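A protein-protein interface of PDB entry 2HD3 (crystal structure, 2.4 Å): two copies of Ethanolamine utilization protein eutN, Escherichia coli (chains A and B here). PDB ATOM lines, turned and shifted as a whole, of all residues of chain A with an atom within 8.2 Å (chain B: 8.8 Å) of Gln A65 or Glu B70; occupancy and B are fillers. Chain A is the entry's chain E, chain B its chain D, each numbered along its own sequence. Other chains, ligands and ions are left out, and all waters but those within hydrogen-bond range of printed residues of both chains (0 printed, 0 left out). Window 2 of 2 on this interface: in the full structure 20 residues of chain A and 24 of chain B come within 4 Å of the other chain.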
ATOM      1  N   VAL A  58      -3.834  -5.299   5.744  1.00  0.00           N
ATOM      2  CA  VAL A  58      -4.566  -4.095   6.085  1.00  0.00           C
ATOM      3  C   VAL A  58      -3.562  -3.308   6.947  1.00  0.00           C
ATOM      4  O   VAL A  58      -2.729  -3.915   7.640  1.00  0.00           O
ATOM      5  CB  VAL A  58      -5.823  -4.419   6.921  1.00  0.00           C
ATOM      6  CG1 VAL A  58      -5.427  -4.950   8.290  1.00  0.00           C
ATOM      7  CG2 VAL A  58      -6.682  -3.179   7.070  1.00  0.00           C
ATOM      8  N   SER A  59      -3.631  -1.976   6.910  1.00  0.00           N
ATOM      9  CA  SER A  59      -2.693  -1.118   7.667  1.00  0.00           C
ATOM     10  C   SER A  59      -3.288   0.135   8.314  1.00  0.00           C
ATOM     11  O   SER A  59      -4.420   0.529   8.026  1.00  0.00           O
ATOM     12  CB  SER A  59      -1.573  -0.650   6.748  1.00  0.00           C
ATOM     13  OG  SER A  59      -2.091   0.231   5.779  1.00  0.00           O
ATOM     14  N   GLY A  60      -2.485   0.779   9.159  1.00  0.00           N
ATOM     15  CA  GLY A  60      -2.920   1.989   9.832  1.00  0.00           C
ATOM     16  C   GLY A  60      -3.897   1.679  10.945  1.00  0.00           C
ATOM     17  O   GLY A  60      -3.770   0.654  11.618  1.00  0.00           O
ATOM     18  N   SER A  61      -4.879   2.554  11.141  1.00  0.00           N
ATOM     19  CA  SER A  61      -5.876   2.354  12.192  1.00  0.00           C
ATOM     20  C   SER A  61      -6.655   1.056  11.997  1.00  0.00           C
ATOM     21  O   SER A  61      -6.895   0.314  12.960  1.00  0.00           O
ATOM     22  CB  SER A  61      -6.851   3.536  12.232  1.00  0.00           C
ATOM     23  OG  SER A  61      -6.723   4.353  11.076  1.00  0.00           O
ATOM     24  N   SER A  62      -7.043   0.790  10.749  1.00  0.00           N
ATOM     25  CA  SER A  62      -7.783  -0.415  10.412  1.00  0.00           C
ATOM     26  C   SER A  62      -6.976  -1.663  10.748  1.00  0.00           C
ATOM     27  O   SER A  62      -7.537  -2.744  10.918  1.00  0.00           O
ATOM     28  CB  SER A  62      -8.149  -0.420   8.925  1.00  0.00           C
ATOM     29  OG  SER A  62      -8.958   0.698   8.592  1.00  0.00           O
ATOM     30  N   ALA A  63      -5.657  -1.530  10.842  1.00  0.00           N
ATOM     31  CA  ALA A  63      -4.836  -2.691  11.175  1.00  0.00           C
ATOM     32  C   ALA A  63      -5.064  -3.035  12.636  1.00  0.00           C
ATOM     33  O   ALA A  63      -5.226  -4.203  12.987  1.00  0.00           O
ATOM     34  CB  ALA A  63      -3.359  -2.398  10.927  1.00  0.00           C
ATOM     35  N   ARG A  64      -5.078  -2.013  13.489  1.00  0.00           N
ATOM     36  CA  ARG A  64      -5.302  -2.236  14.911  1.00  0.00           C
ATOM     37  C   ARG A  64      -6.652  -2.934  15.095  1.00  0.00           C
ATOM     38  O   ARG A  64      -6.728  -3.999  15.707  1.00  0.00           O
ATOM     39  CB  ARG A  64      -5.281  -0.906  15.682  1.00  0.00           C
ATOM     40  CG  ARG A  64      -4.016  -0.071  15.465  1.00  0.00           C
ATOM     41  CD  ARG A  64      -3.923   1.129  16.410  1.00  0.00           C
ATOM     42  NE  ARG A  64      -3.745   2.415  15.720  1.00  0.00           N
ATOM     43  CZ  ARG A  64      -2.724   2.719  14.913  1.00  0.00           C
ATOM     44  NH1 ARG A  64      -2.666   3.919  14.339  1.00  0.00           N
ATOM     45  NH2 ARG A  64      -1.760   1.833  14.669  1.00  0.00           N
ATOM     46  N   GLN A  65      -7.712  -2.349  14.547  1.00  0.00           N
ATOM     47  CA  GLN A  65      -9.041  -2.933  14.676  1.00  0.00           C
ATOM     48  C   GLN A  65      -9.096  -4.378  14.196  1.00  0.00           C
ATOM     49  O   GLN A  65      -9.785  -5.208  14.789  1.00  0.00           O
ATOM     50  CB  GLN A  65     -10.063  -2.099  13.906  1.00  0.00           C
ATOM     51  CG  GLN A  65     -11.114  -1.474  14.803  1.00  0.00           C
ATOM     52  CD  GLN A  65     -10.524  -0.490  15.797  1.00  0.00           C
ATOM     53  OE1 GLN A  65     -10.976  -0.402  16.942  1.00  0.00           O
ATOM     54  NE2 GLN A  65      -9.516   0.263  15.363  1.00  0.00           N
ATOM     55  N   ALA A  66      -8.354  -4.673  13.132  1.00  0.00           N
ATOM     56  CA  ALA A  66      -8.319  -6.014  12.560  1.00  0.00           C
ATOM     57  C   ALA A  66      -7.651  -7.002  13.502  1.00  0.00           C
ATOM     58  O   ALA A  66      -8.017  -8.176  13.548  1.00  0.00           O
ATOM     59  CB  ALA A  66      -7.588  -5.988  11.231  1.00  0.00           C
ATOM     60  N   HIS A  67      -6.660  -6.530  14.252  1.00  0.00           N
ATOM     61  CA  HIS A  67      -5.958  -7.396  15.177  1.00  0.00           C
ATOM     62  C   HIS A  67      -6.714  -7.577  16.480  1.00  0.00           C
ATOM     63  O   HIS A  67      -6.837  -8.696  16.980  1.00  0.00           O
ATOM     64  CB  HIS A  67      -4.566  -6.845  15.473  1.00  0.00           C
ATOM     65  CG  HIS A  67      -3.813  -7.645  16.491  1.00  0.00           C
ATOM     66  ND1 HIS A  67      -3.499  -7.154  17.740  1.00  0.00           N
ATOM     67  CD2 HIS A  67      -3.332  -8.912  16.454  1.00  0.00           C
ATOM     68  CE1 HIS A  67      -2.856  -8.081  18.426  1.00  0.00           C
ATOM     69  NE2 HIS A  67      -2.741  -9.156  17.670  1.00  0.00           N
ATOM     70  N   LYS A  68      -7.231  -6.484  17.028  1.00  0.00           N
ATOM     71  CA  LYS A  68      -7.947  -6.553  18.297  1.00  0.00           C
ATOM     72  C   LYS A  68      -8.786  -5.294  18.526  1.00  0.00           C
ATOM     73  O   LYS A  68      -9.987  -5.298  18.273  1.00  0.00           O
ATOM     74  CB  LYS A  68      -6.927  -6.744  19.427  1.00  0.00           C
ATOM     75  CG  LYS A  68      -7.473  -7.332  20.708  1.00  0.00           C
ATOM     76  CD  LYS A  68      -8.391  -6.370  21.422  1.00  0.00           C
ATOM     77  CE  LYS A  68      -8.710  -6.884  22.819  1.00  0.00           C
ATOM     78  NZ  LYS A  68      -7.472  -7.031  23.638  1.00  0.00           N
ATOM     79  N   SER A  69      -8.160  -4.226  19.015  1.00  0.00           N
ATOM     80  CA  SER A  69      -8.867  -2.970  19.261  1.00  0.00           C
ATOM     81  C   SER A  69      -7.994  -1.761  18.893  1.00  0.00           C
ATOM     82  O   SER A  69      -7.112  -1.873  18.045  1.00  0.00           O
ATOM     83  CB  SER A  69      -9.308  -2.884  20.730  1.00  0.00           C
ATOM     84  OG  SER A  69      -8.202  -2.810  21.604  1.00  0.00           O
ATOM     85  N   GLU A  70      -8.234  -0.610  19.517  1.00  0.00           N
ATOM     86  CA  GLU A  70      -7.440   0.584  19.209  1.00  0.00           C
ATOM     87  C   GLU A  70      -6.147   0.641  20.009  1.00  0.00           C
ATOM     88  O   GLU A  70      -5.299   1.509  19.784  1.00  0.00           O
ATOM     89  CB  GLU A  70      -8.250   1.857  19.464  1.00  0.00           C
ATOM     90  CG  GLU A  70      -8.480   2.706  18.216  1.00  0.00           C
ATOM     91  CD  GLU A  70      -7.194   3.273  17.635  1.00  0.00           C
ATOM     92  OE1 GLU A  70      -6.544   4.092  18.320  1.00  0.00           O
ATOM     93  OE2 GLU A  70      -6.833   2.896  16.495  1.00  0.00           O
ATOM     94  N   THR A  71      -5.999  -0.290  20.945  1.00  0.00           N
ATOM     95  CA  THR A  71      -4.805  -0.341  21.773  1.00  0.00           C
ATOM     96  C   THR A  71      -3.758  -1.287  21.201  1.00  0.00           C
ATOM     97  O   THR A  71      -2.636  -1.341  21.703  1.00  0.00           O
ATOM     98  CB  THR A  71      -5.128  -0.804  23.199  1.00  0.00           C
ATOM     99  OG1 THR A  71      -5.676  -2.125  23.146  1.00  0.00           O
ATOM    100  CG2 THR A  71      -6.122   0.138  23.857  1.00  0.00           C
ATOM    101  N   SER A  72      -4.117  -2.050  20.170  1.00  0.00           N
ATOM    102  CA  SER A  72      -3.142  -2.965  19.582  1.00  0.00           C
ATOM    103  C   SER A  72      -1.999  -2.156  18.987  1.00  0.00           C
ATOM    104  O   SER A  72      -2.223  -1.216  18.220  1.00  0.00           O
ATOM    105  CB  SER A  72      -3.772  -3.839  18.492  1.00  0.00           C
ATOM    106  OG  SER A  72      -4.653  -4.798  19.049  1.00  0.00           O
ATOM    107  N   VAL A  74       0.081  -2.249  16.494  1.00  0.00           N
ATOM    108  CA  VAL A  74       0.428  -2.718  15.153  1.00  0.00           C
ATOM    109  C   VAL A  74      -0.110  -1.793  14.071  1.00  0.00           C
ATOM    110  O   VAL A  74      -1.108  -1.113  14.273  1.00  0.00           O
ATOM    111  CB  VAL A  74      -0.136  -4.127  14.880  1.00  0.00           C
ATOM    112  CG1 VAL A  74       0.514  -5.139  15.800  1.00  0.00           C
ATOM    113  CG2 VAL A  74      -1.647  -4.121  15.070  1.00  0.00           C
ATOM    114  N   CYS A  77      -1.479  -5.856   9.452  1.00  0.00           N
ATOM    115  CA  CYS A  77      -2.104  -7.086   9.887  1.00  0.00           C
ATOM    116  C   CYS A  77      -2.634  -7.938   8.742  1.00  0.00           C
ATOM    117  O   CYS A  77      -3.264  -7.425   7.814  1.00  0.00           O
ATOM    118  CB  CYS A  77      -3.261  -6.750  10.824  1.00  0.00           C
ATOM    119  SG  CYS A  77      -4.028  -8.185  11.591  1.00  0.00           S
ATOM    120  N   ILE A  79      -5.250 -10.111   7.172  1.00  0.00           N
ATOM    121  CA  ILE A  79      -6.693 -10.348   7.353  1.00  0.00           C
ATOM    122  C   ILE A  79      -7.236 -11.472   6.470  1.00  0.00           C
ATOM    123  O   ILE A  79      -8.444 -11.705   6.450  1.00  0.00           O
ATOM    124  CB  ILE A  79      -7.550  -9.095   7.055  1.00  0.00           C
ATOM    125  CG1 ILE A  79      -7.356  -8.662   5.597  1.00  0.00           C
ATOM    126  CG2 ILE A  79      -7.216  -7.990   8.052  1.00  0.00           C
ATOM    127  CD1 ILE A  79      -8.207  -7.459   5.179  1.00  0.00           C
ATOM    128  N   HIS B  16     -10.309 -13.088   7.682  1.00  0.00           N
ATOM    129  CA  HIS B  16     -10.843 -12.516   8.922  1.00  0.00           C
ATOM    130  C   HIS B  16     -12.372 -12.542   8.880  1.00  0.00           C
ATOM    131  O   HIS B  16     -12.972 -12.078   7.913  1.00  0.00           O
ATOM    132  CB  HIS B  16     -10.368 -11.063   9.062  1.00  0.00           C
ATOM    133  CG  HIS B  16     -10.621 -10.449  10.409  1.00  0.00           C
ATOM    134  ND1 HIS B  16     -11.885 -10.188  10.896  1.00  0.00           N
ATOM    135  CD2 HIS B  16      -9.757  -9.981  11.345  1.00  0.00           C
ATOM    136  CE1 HIS B  16     -11.790  -9.580  12.067  1.00  0.00           C
ATOM    137  NE2 HIS B  16     -10.508  -9.443  12.360  1.00  0.00           N
ATOM    138  N   GLY B  18     -14.464 -10.726  10.350  1.00  0.00           N
ATOM    139  CA  GLY B  18     -15.049  -9.395  10.287  1.00  0.00           C
ATOM    140  C   GLY B  18     -15.307  -8.958   8.859  1.00  0.00           C
ATOM    141  O   GLY B  18     -15.891  -7.904   8.615  1.00  0.00           O
ATOM    142  N   GLY B  60      -9.054   4.552   5.041  1.00  0.00           N
ATOM    143  CA  GLY B  60      -8.979   4.836   6.467  1.00  0.00           C
ATOM    144  C   GLY B  60     -10.248   4.482   7.220  1.00  0.00           C
ATOM    145  O   GLY B  60     -10.941   3.527   6.855  1.00  0.00           O
ATOM    146  N   SER B  61     -10.559   5.243   8.269  1.00  0.00           N
ATOM    147  CA  SER B  61     -11.755   4.986   9.064  1.00  0.00           C
ATOM    148  C   SER B  61     -13.000   5.211   8.210  1.00  0.00           C
ATOM    149  O   SER B  61     -14.022   4.552   8.396  1.00  0.00           O
ATOM    150  CB  SER B  61     -11.798   5.890  10.310  1.00  0.00           C
ATOM    151  OG  SER B  61     -12.195   7.219  10.002  1.00  0.00           O
ATOM    152  N   SER B  62     -12.903   6.139   7.265  1.00  0.00           N
ATOM    153  CA  SER B  62     -14.010   6.436   6.376  1.00  0.00           C
ATOM    154  C   SER B  62     -14.405   5.169   5.629  1.00  0.00           C
ATOM    155  O   SER B  62     -15.542   5.030   5.164  1.00  0.00           O
ATOM    156  CB  SER B  62     -13.607   7.522   5.383  1.00  0.00           C
ATOM    157  OG  SER B  62     -13.262   8.713   6.066  1.00  0.00           O
ATOM    158  N   ALA B  63     -13.455   4.246   5.520  1.00  0.00           N
ATOM    159  CA  ALA B  63     -13.683   2.981   4.838  1.00  0.00           C
ATOM    160  C   ALA B  63     -14.368   1.995   5.770  1.00  0.00           C
ATOM    161  O   ALA B  63     -15.368   1.385   5.402  1.00  0.00           O
ATOM    162  CB  ALA B  63     -12.364   2.412   4.344  1.00  0.00           C
ATOM    163  N   ARG B  64     -13.839   1.844   6.980  1.00  0.00           N
ATOM    164  CA  ARG B  64     -14.432   0.926   7.942  1.00  0.00           C
ATOM    165  C   ARG B  64     -15.922   1.209   8.096  1.00  0.00           C
ATOM    166  O   ARG B  64     -16.746   0.299   8.005  1.00  0.00           O
ATOM    167  CB  ARG B  64     -13.746   1.044   9.304  1.00  0.00           C
ATOM    168  CG  ARG B  64     -12.289   0.607   9.303  1.00  0.00           C
ATOM    169  CD  ARG B  64     -11.774   0.371  10.713  1.00  0.00           C
ATOM    170  NE  ARG B  64     -11.674   1.595  11.506  1.00  0.00           N
ATOM    171  CZ  ARG B  64     -10.678   2.473  11.416  1.00  0.00           C
ATOM    172  NH1 ARG B  64     -10.684   3.558  12.182  1.00  0.00           N
ATOM    173  NH2 ARG B  64      -9.675   2.266  10.568  1.00  0.00           N
ATOM    174  N   GLN B  65     -16.268   2.471   8.327  1.00  0.00           N
ATOM    175  CA  GLN B  65     -17.667   2.846   8.482  1.00  0.00           C
ATOM    176  C   GLN B  65     -18.439   2.547   7.202  1.00  0.00           C
ATOM    177  O   GLN B  65     -19.475   1.880   7.229  1.00  0.00           O
ATOM    178  CB  GLN B  65     -17.784   4.334   8.829  1.00  0.00           C
ATOM    179  CG  GLN B  65     -17.642   4.638  10.310  1.00  0.00           C
ATOM    180  CD  GLN B  65     -18.750   4.007  11.142  1.00  0.00           C
ATOM    181  OE1 GLN B  65     -18.871   2.783  11.210  1.00  0.00           O
ATOM    182  NE2 GLN B  65     -19.568   4.844  11.774  1.00  0.00           N
ATOM    183  N   ALA B  66     -17.921   3.033   6.080  1.00  0.00           N
ATOM    184  CA  ALA B  66     -18.561   2.815   4.795  1.00  0.00           C
ATOM    185  C   ALA B  66     -18.748   1.319   4.532  1.00  0.00           C
ATOM    186  O   ALA B  66     -19.503   0.929   3.647  1.00  0.00           O
ATOM    187  CB  ALA B  66     -17.730   3.450   3.687  1.00  0.00           C
ATOM    188  N   HIS B  67     -18.061   0.481   5.303  1.00  0.00           N
ATOM    189  CA  HIS B  67     -18.183  -0.963   5.128  1.00  0.00           C
ATOM    190  C   HIS B  67     -19.305  -1.530   5.987  1.00  0.00           C
ATOM    191  O   HIS B  67     -20.321  -1.986   5.470  1.00  0.00           O
ATOM    192  CB  HIS B  67     -16.878  -1.672   5.485  1.00  0.00           C
ATOM    193  CG  HIS B  67     -16.962  -3.162   5.383  1.00  0.00           C
ATOM    194  ND1 HIS B  67     -16.552  -4.003   6.393  1.00  0.00           N
ATOM    195  CD2 HIS B  67     -17.417  -3.962   4.390  1.00  0.00           C
ATOM    196  CE1 HIS B  67     -16.751  -5.255   6.029  1.00  0.00           C
ATOM    197  NE2 HIS B  67     -17.275  -5.259   4.817  1.00  0.00           N
ATOM    198  N   LYS B  68     -19.108  -1.502   7.299  1.00  0.00           N
ATOM    199  CA  LYS B  68     -20.090  -2.022   8.244  1.00  0.00           C
ATOM    200  C   LYS B  68     -20.103  -1.162   9.498  1.00  0.00           C
ATOM    201  O   LYS B  68     -21.161  -0.727   9.949  1.00  0.00           O
ATOM    202  CB  LYS B  68     -19.746  -3.476   8.606  1.00  0.00           C
ATOM    203  CG  LYS B  68     -20.495  -4.033   9.808  1.00  0.00           C
ATOM    204  CD  LYS B  68     -21.983  -4.137   9.543  1.00  0.00           C
ATOM    205  CE  LYS B  68     -22.757  -4.517  10.803  1.00  0.00           C
ATOM    206  NZ  LYS B  68     -22.721  -3.453  11.849  1.00  0.00           N
ATOM    207  N   SER B  69     -18.914  -0.914  10.044  1.00  0.00           N
ATOM    208  CA  SER B  69     -18.762  -0.111  11.254  1.00  0.00           C
ATOM    209  C   SER B  69     -17.298   0.235  11.541  1.00  0.00           C
ATOM    210  O   SER B  69     -16.437   0.177  10.659  1.00  0.00           O
ATOM    211  CB  SER B  69     -19.324  -0.871  12.457  1.00  0.00           C
ATOM    212  OG  SER B  69     -18.560  -2.044  12.704  1.00  0.00           O
ATOM    213  N   GLU B  70     -17.034   0.590  12.797  1.00  0.00           N
ATOM    214  CA  GLU B  70     -15.698   0.933  13.257  1.00  0.00           C
ATOM    215  C   GLU B  70     -14.918  -0.326  13.590  1.00  0.00           C
ATOM    216  O   GLU B  70     -13.782  -0.254  14.045  1.00  0.00           O
ATOM    217  CB  GLU B  70     -15.784   1.811  14.503  1.00  0.00           C
ATOM    218  CG  GLU B  70     -15.519   3.282  14.250  1.00  0.00           C
ATOM    219  CD  GLU B  70     -14.084   3.538  13.846  1.00  0.00           C
ATOM    220  OE1 GLU B  70     -13.175   3.225  14.652  1.00  0.00           O
ATOM    221  OE2 GLU B  70     -13.864   4.048  12.727  1.00  0.00           O
ATOM    222  N   THR B  71     -15.534  -1.479  13.360  1.00  0.00           N
ATOM    223  CA  THR B  71     -14.906  -2.761  13.646  1.00  0.00           C
ATOM    224  C   THR B  71     -14.328  -3.363  12.376  1.00  0.00           C
ATOM    225  O   THR B  71     -13.408  -4.186  12.427  1.00  0.00           O
ATOM    226  CB  THR B  71     -15.931  -3.774  14.204  1.00  0.00           C
ATOM    227  OG1 THR B  71     -16.848  -3.102  15.074  1.00  0.00           O
ATOM    228  CG2 THR B  71     -15.218  -4.878  14.977  1.00  0.00           C
ATOM    229  N   SER B  72     -14.892  -2.960  11.240  1.00  0.00           N
ATOM    230  CA  SER B  72     -14.469  -3.460   9.933  1.00  0.00           C
ATOM    231  C   SER B  72     -12.954  -3.433   9.754  1.00  0.00           C
ATOM    232  O   SER B  72     -12.318  -2.381   9.870  1.00  0.00           O
ATOM    233  CB  SER B  72     -15.133  -2.640   8.825  1.00  0.00           C
ATOM    234  OG  SER B  72     -16.551  -2.654   8.962  1.00  0.00           O
ATOM    235  N   PRO B  73     -12.359  -4.598   9.471  1.00  0.00           N
ATOM    236  CA  PRO B  73     -10.912  -4.716   9.276  1.00  0.00           C
ATOM    237  C   PRO B  73     -10.464  -4.321   7.869  1.00  0.00           C
ATOM    238  O   PRO B  73      -9.774  -5.091   7.202  1.00  0.00           O
ATOM    239  CB  PRO B  73     -10.663  -6.187   9.562  1.00  0.00           C
ATOM    240  CG  PRO B  73     -11.877  -6.828   8.962  1.00  0.00           C
ATOM    241  CD  PRO B  73     -12.998  -5.928   9.453  1.00  0.00           C
ATOM    242  N   VAL B  74     -10.846  -3.127   7.420  1.00  0.00           N
ATOM    243  CA  VAL B  74     -10.482  -2.669   6.080  1.00  0.00           C
ATOM    244  C   VAL B  74      -9.969  -1.229   6.023  1.00  0.00           C
ATOM    245  O   VAL B  74     -10.321  -0.394   6.850  1.00  0.00           O
ATOM    246  CB  VAL B  74     -11.686  -2.767   5.104  1.00  0.00           C
ATOM    247  CG1 VAL B  74     -12.281  -4.155   5.150  1.00  0.00           C
ATOM    248  CG2 VAL B  74     -12.739  -1.710   5.448  1.00  0.00           C
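Ser A61 touches Arg B64, but with the chains exchanged Arg A64 does not touch Ser B61 (10.0 Å).
Ser A62 touches Gly B60, but with the chains exchanged Gly A60 does not touch Ser B62 (10.7 Å).
Ser A62 touches Arg B64, but with the chains exchanged Arg A64 does not touch Ser B62 (12.6 Å).
Ser A62 touches Val B74, but with the chains exchanged Val A74 does not touch Ser B62 (15.5 Å).
NE2 of His B16 sits at hydrogen-bond distance from O of Ala A66, at 3.0 Å.
The backbone carbonyl oxygen of Val B74 is in hydrogen-bond range of the side-chain hydroxyl of Ser A62 (2.5 Å).
N of His B16 sits at hydrogen-bond distance from O of Ile A79, 2.6 Å away.
The guanidinium group of Arg B64 sits at hydrogen-bond distance from the side-chain hydroxyl of Ser A62, 2.6 Å away.
Among the printed residues, merely in contact across the chains: Val A58 with Pro B73, Val A58 with Val B74, Ser A61 with Arg B64, Ser A62 with Gly B60, Gln A65 with Glu B70, Ala A66 with Pro B73 and Ile A79 with Pro B73.
Of the 18 printed residues of chain A, 6 touch a printed residue of chain B.
Hydrophobic or aromatic side chains of chain A that line the printed part of chain B: Val A58, Ala A66 and Ile A79.
Along chain A the printed residues that touch a printed residue of chain B span positions 58 to 79.
Of the 17 printed residues of chain B, 6 touch a printed residue of chain A.
Printed residues of chain B that touch a printed residue of chain A: His B16, Gly B60, Arg B64, Glu B70, Pro B73 and Val B74.
Among the printed residues, 11 pairs touch across the chains.
Among the printed residues, no Asp or Glu carboxylate lies within 4 Å of a Lys or Arg side-chain nitrogen of the other chain.
The guanidinium group (NH1) of Arg B64 lies within salt-bridge range of the side-chain carboxylate (OE2) of Glu B70.
O of Val A58 lies within hydrogen-bond range of N of Cys A77, 2.9 Å away.
ND1 of His B16 sits at hydrogen-bond distance from N of Gly B18 (2.7 Å).
OE1 of Gln B65 is in hydrogen-bond range of N of Glu B70, at 3.3 Å.
The backbone NH (N) of Ser B69 lies within hydrogen-bond range of the backbone carbonyl oxygen (O) of Arg B64 (3.2 Å).
The backbone carbonyl oxygen (O) of Arg B64 is in hydrogen-bond range of the side-chain hydroxyl (OG) of Ser B72 (3.1 Å).
Gln A65 touches one residue of chain B.
Of chain A, only Gln A65 comes within 4 Å of Glu B70.
Printed residues of chain B within 4 Å of Ala A66: His B16 and Pro B73.
No residue of chain A comes within 4 Å of Ser B69.
Of the printed residues of chain B, Ser A61 touches Arg B64 (3.5 Å).
Of the printed residues of chain A, Val B74 touches Val A58 (3.96 Å) and Ser A62 (2.5 Å).
Lys B68 touches none of the printed residues of chain A.
The nearest residue of chain B that does not touch Gln A65 is Thr B71 (4.2 Å).
The nearest printed residue of chain A that does not touch Gly B60 is Ser A61 (5.2 Å).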
